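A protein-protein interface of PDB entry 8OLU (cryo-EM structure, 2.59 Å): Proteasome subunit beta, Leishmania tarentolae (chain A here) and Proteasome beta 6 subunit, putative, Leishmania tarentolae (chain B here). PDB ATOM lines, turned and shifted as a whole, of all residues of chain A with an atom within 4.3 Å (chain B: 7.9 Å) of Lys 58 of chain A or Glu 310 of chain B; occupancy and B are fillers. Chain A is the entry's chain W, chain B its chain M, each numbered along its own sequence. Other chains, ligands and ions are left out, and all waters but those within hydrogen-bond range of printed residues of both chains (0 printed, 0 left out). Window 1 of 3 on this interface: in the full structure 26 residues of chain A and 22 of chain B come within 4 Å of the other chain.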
ATOM      1  N   THR A  47      11.215 -20.364   3.771  1.00  0.00           N
ATOM      2  CA  THR A  47      11.144 -20.387   5.211  1.00  0.00           C
ATOM      3  C   THR A  47      10.004 -19.570   5.777  1.00  0.00           C
ATOM      4  O   THR A  47       9.906 -19.440   6.956  1.00  0.00           O
ATOM      5  CB  THR A  47      12.435 -19.859   5.813  1.00  0.00           C
ATOM      6  OG1 THR A  47      12.508 -18.448   5.555  1.00  0.00           O
ATOM      7  CG2 THR A  47      13.651 -20.582   5.275  1.00  0.00           C
ATOM      8  N   ARG A  48       9.056 -19.126   5.021  1.00  0.00           N
ATOM      9  CA  ARG A  48       8.001 -18.404   5.693  1.00  0.00           C
ATOM     10  C   ARG A  48       6.954 -19.352   6.235  1.00  0.00           C
ATOM     11  O   ARG A  48       6.227 -19.971   5.470  1.00  0.00           O
ATOM     12  CB  ARG A  48       7.357 -17.483   4.665  1.00  0.00           C
ATOM     13  CG  ARG A  48       6.056 -16.830   5.081  1.00  0.00           C
ATOM     14  CD  ARG A  48       5.474 -16.081   3.886  1.00  0.00           C
ATOM     15  NE  ARG A  48       6.330 -14.938   3.704  1.00  0.00           N
ATOM     16  CZ  ARG A  48       6.131 -14.020   2.784  1.00  0.00           C
ATOM     17  NH1 ARG A  48       5.043 -14.004   2.015  1.00  0.00           N
ATOM     18  NH2 ARG A  48       7.072 -13.111   2.659  1.00  0.00           N
ATOM     19  N   VAL A  55       2.612 -13.612   8.569  1.00  0.00           N
ATOM     20  CA  VAL A  55       3.831 -14.356   8.729  1.00  0.00           C
ATOM     21  C   VAL A  55       4.188 -14.527  10.194  1.00  0.00           C
ATOM     22  O   VAL A  55       4.788 -13.657  10.829  1.00  0.00           O
ATOM     23  CB  VAL A  55       4.912 -13.590   7.959  1.00  0.00           C
ATOM     24  CG1 VAL A  55       6.257 -14.225   8.100  1.00  0.00           C
ATOM     25  CG2 VAL A  55       4.502 -13.440   6.498  1.00  0.00           C
ATOM     26  N   ASP A  57       6.313 -16.672  11.437  1.00  0.00           N
ATOM     27  CA  ASP A  57       7.748 -16.858  11.558  1.00  0.00           C
ATOM     28  C   ASP A  57       8.345 -16.650  10.188  1.00  0.00           C
ATOM     29  O   ASP A  57       7.945 -17.275   9.234  1.00  0.00           O
ATOM     30  CB  ASP A  57       8.167 -18.233  12.095  1.00  0.00           C
ATOM     31  CG  ASP A  57       9.668 -18.351  12.381  1.00  0.00           C
ATOM     32  OD1 ASP A  57      10.400 -17.319  12.162  1.00  0.00           O
ATOM     33  OD2 ASP A  57      10.117 -19.466  12.863  1.00  0.00           O
ATOM     34  N   LYS A  58       9.349 -15.807  10.154  1.00  0.00           N
ATOM     35  CA  LYS A  58       9.985 -15.460   8.915  1.00  0.00           C
ATOM     36  C   LYS A  58      10.946 -16.569   8.553  1.00  0.00           C
ATOM     37  O   LYS A  58      11.128 -16.795   7.369  1.00  0.00           O
ATOM     38  CB  LYS A  58      10.613 -14.076   9.052  1.00  0.00           C
ATOM     39  CG  LYS A  58       9.624 -12.957   8.731  1.00  0.00           C
ATOM     40  CD  LYS A  58      10.126 -11.537   8.942  1.00  0.00           C
ATOM     41  CE  LYS A  58      10.411 -11.227  10.399  1.00  0.00           C
ATOM     42  NZ  LYS A  58      10.415  -9.764  10.622  1.00  0.00           N
ATOM     43  N   ARG A  59      11.488 -17.290   9.536  1.00  0.00           N
ATOM     44  CA  ARG A  59      12.630 -18.146   9.285  1.00  0.00           C
ATOM     45  C   ARG A  59      12.447 -19.538   9.870  1.00  0.00           C
ATOM     46  O   ARG A  59      13.370 -20.039  10.512  1.00  0.00           O
ATOM     47  CB  ARG A  59      13.905 -17.550   9.874  1.00  0.00           C
ATOM     48  CG  ARG A  59      14.571 -16.549   8.939  1.00  0.00           C
ATOM     49  CD  ARG A  59      15.925 -16.022   9.410  1.00  0.00           C
ATOM     50  NE  ARG A  59      15.798 -15.145  10.571  1.00  0.00           N
ATOM     51  CZ  ARG A  59      15.243 -13.929  10.556  1.00  0.00           C
ATOM     52  NH1 ARG A  59      14.834 -13.385  11.691  1.00  0.00           N
ATOM     53  NH2 ARG A  59      15.099 -13.273   9.413  1.00  0.00           N
ATOM     54  N   CYS A  60      11.337 -20.224   9.576  1.00  0.00           N
ATOM     55  CA  CYS A  60      11.250 -21.583  10.082  1.00  0.00           C
ATOM     56  C   CYS A  60      11.974 -22.571   9.169  1.00  0.00           C
ATOM     57  O   CYS A  60      12.125 -22.306   7.985  1.00  0.00           O
ATOM     58  CB  CYS A  60       9.832 -22.065  10.299  1.00  0.00           C
ATOM     59  SG  CYS A  60       8.949 -22.145   8.743  1.00  0.00           S
ATOM     60  N   THR A 200      10.850 -15.320   2.280  1.00  0.00           N
ATOM     61  CA  THR A 200      11.985 -14.993   3.102  1.00  0.00           C
ATOM     62  C   THR A 200      13.257 -15.435   2.431  1.00  0.00           C
ATOM     63  O   THR A 200      13.920 -14.588   1.848  1.00  0.00           O
ATOM     64  CB  THR A 200      11.994 -15.520   4.530  1.00  0.00           C
ATOM     65  OG1 THR A 200      10.772 -15.360   5.254  1.00  0.00           O
ATOM     66  CG2 THR A 200      13.090 -14.802   5.288  1.00  0.00           C
ATOM     67  N   ARG A 224      15.918  -6.220   4.909  1.00  0.00           N
ATOM     68  CA  ARG A 224      14.886  -5.185   4.980  1.00  0.00           C
ATOM     69  C   ARG A 224      15.500  -3.837   4.577  1.00  0.00           C
ATOM     70  O   ARG A 224      16.660  -3.553   4.877  1.00  0.00           O
ATOM     71  CB  ARG A 224      14.161  -5.172   6.336  1.00  0.00           C
ATOM     72  CG  ARG A 224      14.989  -4.761   7.548  1.00  0.00           C
ATOM     73  CD  ARG A 224      14.104  -4.695   8.789  1.00  0.00           C
ATOM     74  NE  ARG A 224      13.117  -3.615   8.754  1.00  0.00           N
ATOM     75  CZ  ARG A 224      12.086  -3.485   9.592  1.00  0.00           C
ATOM     76  NH1 ARG A 224      11.703  -2.287  10.002  1.00  0.00           N
ATOM     77  NH2 ARG A 224      11.449  -4.549  10.046  1.00  0.00           N
ATOM     78  N   PHE B 270      -2.930  -4.111  11.291  1.00  0.00           N
ATOM     79  CA  PHE B 270      -1.603  -4.071  11.875  1.00  0.00           C
ATOM     80  C   PHE B 270      -1.136  -2.657  12.090  1.00  0.00           C
ATOM     81  O   PHE B 270      -0.471  -2.344  13.080  1.00  0.00           O
ATOM     82  CB  PHE B 270      -0.442  -4.312  10.914  1.00  0.00           C
ATOM     83  CG  PHE B 270      -0.340  -5.708  10.448  1.00  0.00           C
ATOM     84  CD1 PHE B 270      -1.118  -6.697  10.997  1.00  0.00           C
ATOM     85  CD2 PHE B 270       0.535  -6.023   9.453  1.00  0.00           C
ATOM     86  CE1 PHE B 270      -1.025  -8.012  10.577  1.00  0.00           C
ATOM     87  CE2 PHE B 270       0.589  -7.331   8.995  1.00  0.00           C
ATOM     88  CZ  PHE B 270      -0.184  -8.328   9.562  1.00  0.00           C
ATOM     89  N   ASN B 303       7.890   3.413   8.309  1.00  0.00           N
ATOM     90  CA  ASN B 303       8.242   2.387   9.257  1.00  0.00           C
ATOM     91  C   ASN B 303       7.075   1.405   9.323  1.00  0.00           C
ATOM     92  O   ASN B 303       7.271   0.208   9.559  1.00  0.00           O
ATOM     93  CB  ASN B 303       8.624   2.956  10.611  1.00  0.00           C
ATOM     94  CG  ASN B 303       8.922   1.841  11.598  1.00  0.00           C
ATOM     95  OD1 ASN B 303       9.946   1.175  11.459  1.00  0.00           O
ATOM     96  ND2 ASN B 303       8.043   1.587  12.569  1.00  0.00           N
ATOM     97  N   ALA B 304       5.860   1.875   9.085  1.00  0.00           N
ATOM     98  CA  ALA B 304       4.712   1.042   9.396  1.00  0.00           C
ATOM     99  C   ALA B 304       4.286   0.232   8.164  1.00  0.00           C
ATOM    100  O   ALA B 304       3.858  -0.911   8.291  1.00  0.00           O
ATOM    101  CB  ALA B 304       3.580   1.886   9.922  1.00  0.00           C
ATOM    102  N   PHE B 305       4.412   0.805   6.978  1.00  0.00           N
ATOM    103  CA  PHE B 305       4.417   0.027   5.755  1.00  0.00           C
ATOM    104  C   PHE B 305       5.513  -1.018   5.742  1.00  0.00           C
ATOM    105  O   PHE B 305       5.314  -2.114   5.261  1.00  0.00           O
ATOM    106  CB  PHE B 305       4.624   0.920   4.536  1.00  0.00           C
ATOM    107  CG  PHE B 305       3.271   1.257   4.002  1.00  0.00           C
ATOM    108  CD1 PHE B 305       2.661   0.409   3.102  1.00  0.00           C
ATOM    109  CD2 PHE B 305       2.549   2.292   4.553  1.00  0.00           C
ATOM    110  CE1 PHE B 305       1.373   0.675   2.660  1.00  0.00           C
ATOM    111  CE2 PHE B 305       1.262   2.542   4.136  1.00  0.00           C
ATOM    112  CZ  PHE B 305       0.674   1.741   3.173  1.00  0.00           C
ATOM    113  N   THR B 306       6.673  -0.678   6.258  1.00  0.00           N
ATOM    114  CA  THR B 306       7.776  -1.605   6.188  1.00  0.00           C
ATOM    115  C   THR B 306       7.477  -2.842   7.008  1.00  0.00           C
ATOM    116  O   THR B 306       7.562  -3.922   6.455  1.00  0.00           O
ATOM    117  CB  THR B 306       9.077  -0.962   6.635  1.00  0.00           C
ATOM    118  OG1 THR B 306       9.455  -0.085   5.574  1.00  0.00           O
ATOM    119  CG2 THR B 306      10.110  -2.022   6.874  1.00  0.00           C
ATOM    120  N   GLY B 307       7.101  -2.674   8.274  1.00  0.00           N
ATOM    121  CA  GLY B 307       6.618  -3.762   9.104  1.00  0.00           C
ATOM    122  C   GLY B 307       5.420  -4.478   8.496  1.00  0.00           C
ATOM    123  O   GLY B 307       5.298  -5.688   8.573  1.00  0.00           O
ATOM    124  N   ALA B 308       4.491  -3.793   7.863  1.00  0.00           N
ATOM    125  CA  ALA B 308       3.388  -4.555   7.292  1.00  0.00           C
ATOM    126  C   ALA B 308       3.848  -5.455   6.142  1.00  0.00           C
ATOM    127  O   ALA B 308       3.307  -6.528   5.945  1.00  0.00           O
ATOM    128  CB  ALA B 308       2.334  -3.630   6.744  1.00  0.00           C
ATOM    129  N   ALA B 309       4.705  -4.950   5.263  1.00  0.00           N
ATOM    130  CA  ALA B 309       5.164  -5.757   4.159  1.00  0.00           C
ATOM    131  C   ALA B 309       5.767  -7.041   4.701  1.00  0.00           C
ATOM    132  O   ALA B 309       5.509  -8.106   4.121  1.00  0.00           O
ATOM    133  CB  ALA B 309       6.174  -5.023   3.331  1.00  0.00           C
ATOM    134  N   GLU B 310       6.464  -6.941   5.834  1.00  0.00           N
ATOM    135  CA  GLU B 310       7.052  -8.121   6.439  1.00  0.00           C
ATOM    136  C   GLU B 310       6.047  -9.195   6.833  1.00  0.00           C
ATOM    137  O   GLU B 310       6.448 -10.337   7.002  1.00  0.00           O
ATOM    138  CB  GLU B 310       7.692  -7.898   7.815  1.00  0.00           C
ATOM    139  CG  GLU B 310       8.901  -6.979   7.858  1.00  0.00           C
ATOM    140  CD  GLU B 310      10.086  -7.273   6.949  1.00  0.00           C
ATOM    141  OE1 GLU B 310      10.377  -6.406   6.067  1.00  0.00           O
ATOM    142  OE2 GLU B 310      10.762  -8.322   7.170  1.00  0.00           O
ATOM    143  N   ARG B 311       4.819  -8.823   7.176  1.00  0.00           N
ATOM    144  CA  ARG B 311       3.969  -9.716   7.940  1.00  0.00           C
ATOM    145  C   ARG B 311       2.646  -9.958   7.265  1.00  0.00           C
ATOM    146  O   ARG B 311       2.045 -10.969   7.490  1.00  0.00           O
ATOM    147  CB  ARG B 311       3.703  -9.171   9.328  1.00  0.00           C
ATOM    148  CG  ARG B 311       4.985  -9.120  10.142  1.00  0.00           C
ATOM    149  CD  ARG B 311       5.109 -10.295  11.054  1.00  0.00           C
ATOM    150  NE  ARG B 311       6.451 -10.326  11.584  1.00  0.00           N
ATOM    151  CZ  ARG B 311       6.902 -11.333  12.309  1.00  0.00           C
ATOM    152  NH1 ARG B 311       6.234 -12.482  12.328  1.00  0.00           N
ATOM    153  NH2 ARG B 311       7.962 -11.152  13.078  1.00  0.00           N
ATOM    154  N   ASP B 312       2.175  -9.028   6.460  1.00  0.00           N
ATOM    155  CA  ASP B 312       1.006  -9.299   5.667  1.00  0.00           C
ATOM    156  C   ASP B 312       1.492  -9.784   4.317  1.00  0.00           C
ATOM    157  O   ASP B 312       2.234  -9.101   3.587  1.00  0.00           O
ATOM    158  CB  ASP B 312       0.133  -8.055   5.574  1.00  0.00           C
ATOM    159  CG  ASP B 312      -0.964  -8.118   4.508  1.00  0.00           C
ATOM    160  OD1 ASP B 312      -1.692  -9.186   4.432  1.00  0.00           O
ATOM    161  OD2 ASP B 312      -1.109  -7.091   3.763  1.00  0.00           O
ATOM    162  N   ILE B 313       1.052 -10.975   3.975  1.00  0.00           N
ATOM    163  CA  ILE B 313       1.556 -11.532   2.756  1.00  0.00           C
ATOM    164  C   ILE B 313       0.975 -10.852   1.533  1.00  0.00           C
ATOM    165  O   ILE B 313       1.502 -11.101   0.463  1.00  0.00           O
ATOM    166  CB  ILE B 313       1.280 -13.015   2.703  1.00  0.00           C
ATOM    167  CG1 ILE B 313      -0.205 -13.250   2.486  1.00  0.00           C
ATOM    168  CG2 ILE B 313       1.833 -13.701   3.932  1.00  0.00           C
ATOM    169  CD1 ILE B 313      -0.634 -14.586   3.023  1.00  0.00           C
ATOM    170  N   THR B 315       0.628  -7.460   1.170  1.00  0.00           N
ATOM    171  CA  THR B 315       1.207  -6.140   1.018  1.00  0.00           C
ATOM    172  C   THR B 315       2.681  -6.353   0.769  1.00  0.00           C
ATOM    173  O   THR B 315       3.290  -7.187   1.423  1.00  0.00           O
ATOM    174  CB  THR B 315       0.917  -5.251   2.239  1.00  0.00           C
ATOM    175  OG1 THR B 315      -0.394  -4.709   2.024  1.00  0.00           O
ATOM    176  CG2 THR B 315       1.917  -4.115   2.418  1.00  0.00           C
ATOM    177  N   GLY B 316       3.215  -5.585  -0.161  1.00  0.00           N
ATOM    178  CA  GLY B 316       4.639  -5.585  -0.402  1.00  0.00           C
ATOM    179  C   GLY B 316       4.929  -4.724  -1.620  1.00  0.00           C
ATOM    180  O   GLY B 316       4.061  -3.970  -2.067  1.00  0.00           O
ATOM    181  N   LEU B 336       9.446  -1.625  -0.665  1.00  0.00           N
ATOM    182  CA  LEU B 336       9.160  -2.652   0.313  1.00  0.00           C
ATOM    183  C   LEU B 336       9.736  -3.991  -0.142  1.00  0.00           C
ATOM    184  O   LEU B 336      10.120  -4.158  -1.298  1.00  0.00           O
ATOM    185  CB  LEU B 336       7.646  -2.842   0.418  1.00  0.00           C
ATOM    186  CG  LEU B 336       6.835  -1.637   0.855  1.00  0.00           C
ATOM    187  CD1 LEU B 336       5.385  -2.041   1.140  1.00  0.00           C
ATOM    188  CD2 LEU B 336       7.486  -1.007   2.064  1.00  0.00           C
ATOM    189  N   ARG B 337       9.700  -4.981   0.737  1.00  0.00           N
ATOM    190  CA  ARG B 337      10.306  -6.249   0.380  1.00  0.00           C
ATOM    191  C   ARG B 337       9.377  -7.037  -0.542  1.00  0.00           C
ATOM    192  O   ARG B 337       8.242  -7.323  -0.175  1.00  0.00           O
ATOM    193  CB  ARG B 337      10.713  -7.050   1.625  1.00  0.00           C
ATOM    194  CG  ARG B 337       9.552  -7.709   2.353  1.00  0.00           C
ATOM    195  CD  ARG B 337      10.148  -8.388   3.564  1.00  0.00           C
ATOM    196  NE  ARG B 337      10.761  -9.682   3.322  1.00  0.00           N
ATOM    197  CZ  ARG B 337      11.381 -10.376   4.261  1.00  0.00           C
ATOM    198  NH1 ARG B 337      11.239 -11.690   4.334  1.00  0.00           N
ATOM    199  NH2 ARG B 337      12.059  -9.728   5.187  1.00  0.00           N
ATOM    200  N   LYS B 338       9.986  -7.519  -1.633  1.00  0.00           N
ATOM    201  CA  LYS B 338       9.334  -8.100  -2.786  1.00  0.00           C
ATOM    202  C   LYS B 338       8.662  -9.447  -2.525  1.00  0.00           C
ATOM    203  O   LYS B 338       7.719  -9.779  -3.238  1.00  0.00           O
ATOM    204  CB  LYS B 338      10.343  -8.297  -3.914  1.00  0.00           C
ATOM    205  CG  LYS B 338      11.155  -7.072  -4.280  1.00  0.00           C
ATOM    206  CD  LYS B 338      10.344  -5.917  -4.813  1.00  0.00           C
ATOM    207  CE  LYS B 338      11.224  -4.704  -5.047  1.00  0.00           C
ATOM    208  NZ  LYS B 338      10.443  -3.448  -4.962  1.00  0.00           N
ATOM    209  N   ASP B 339       9.080 -10.242  -1.540  1.00  0.00           N
ATOM    210  CA  ASP B 339       8.446 -11.551  -1.325  1.00  0.00           C
ATOM    211  C   ASP B 339       6.986 -11.475  -0.791  1.00  0.00           C
ATOM    212  O   ASP B 339       6.534 -10.348  -0.419  1.00  0.00           O
ATOM    213  CB  ASP B 339       9.300 -12.438  -0.412  1.00  0.00           C
ATOM    214  CG  ASP B 339       9.413 -11.991   1.035  1.00  0.00           C
ATOM    215  OD1 ASP B 339       8.778 -10.962   1.406  1.00  0.00           O
ATOM    216  OD2 ASP B 339      10.137 -12.673   1.790  1.00  0.00           O
ATOM    217  OXT ASP B 339       6.318 -12.571  -0.746  1.00  0.00           O
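Printed residues of chain B that touch a printed residue of chain A: Thr 306, Glu 310, Arg 311, Ile 313, Arg 337 and Asp 339.
Hydrophobic or aromatic side chains of chain B within 4 Å of the printed part of chain A: Ile 313.
Of the 9 printed residues of chain A, 5 touch a printed residue of chain B.
Hydrophobic or aromatic side chains of chain A that line the printed part of chain B: Val 55.
Among the printed residues, 11 pairs touch across the chains.
Among the printed residues, Asp or Glu carboxylates within 4 Å of a Lys or Arg side-chain nitrogen of the other chain: Arg 48 of chain A with Asp 339 of chain B (3.0 Å) and Lys 58 of chain A with Glu 310 of chain B (3.8 Å).
OG1 of Thr 200 of chain A is in hydrogen-bond range of O of Lys 58 of chain A, at 2.6 Å.
The side-chain carboxylate of Glu 310 of chain B lies within salt-bridge range of the guanidinium group of Arg 337 of chain B (2.8 Å).
NH1 of Arg 337 of chain B is in salt-bridge range of OD2 of Asp 339 of chain B.
The backbone carbonyl oxygen (O) of Lys 58 of chain A is in hydrogen-bond range of the side-chain hydroxyl (OG1) of Thr 47 of chain A, 2.8 Å away.
OD1 of Asp 339 of chain B lies within salt-bridge range of NH2 of Arg 48 of chain A (3.0 Å).
The backbone NH (N) of Thr 200 of chain A lies within hydrogen-bond range of the side-chain carboxylate (OD2) of Asp 339 of chain B (2.8 Å).
O of Arg 311 of chain B sits at hydrogen-bond distance from N of Val 55 of chain A (2.9 Å).
The side-chain carboxylate (OE2) of Glu 310 of chain B is in salt-bridge range of the side-chain amino group (NZ) of Lys 58 of chain A (3.8 Å).
Among the printed residues, merely in contact across the chains: Arg 224 of chain A with Thr 306 of chain B (3.5 Å), Thr 200 of chain A with Arg 337 of chain B (3.6 Å), Lys 58 of chain A with Arg 311 of chain B (3.6 Å), Val 55 of chain A with Glu 310 of chain B (3.7 Å), Val 55 of chain A with Ile 313 of chain B (3.7 Å), Arg 48 of chain A with Ile 313 of chain B (3.8 Å) and Arg 224 of chain A with Glu 310 of chain B (3.99 Å).
Of the printed residues of chain B, Lys 58 of chain A touches Glu 310 and Arg 311.
Printed residues of chain A within 4 Å of Glu 310 of chain B: Val 55, Lys 58 and Arg 224.
Printed residues of chain B within 4 Å of Val 55 of chain A: Glu 310 (3.7 Å), Arg 311 (2.4 Å) and Ile 313 (3.7 Å).
Printed residues of chain A within 4 Å of Asp 339 of chain B: Arg 48 and Thr 200.
Printed residues of chain B within 4 Å of Thr 200 of chain A: Arg 337 and Asp 339.
The nearest printed residue of chain B that does not touch Thr 200 of chain A is Glu 310 of chain B (6.9 Å).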
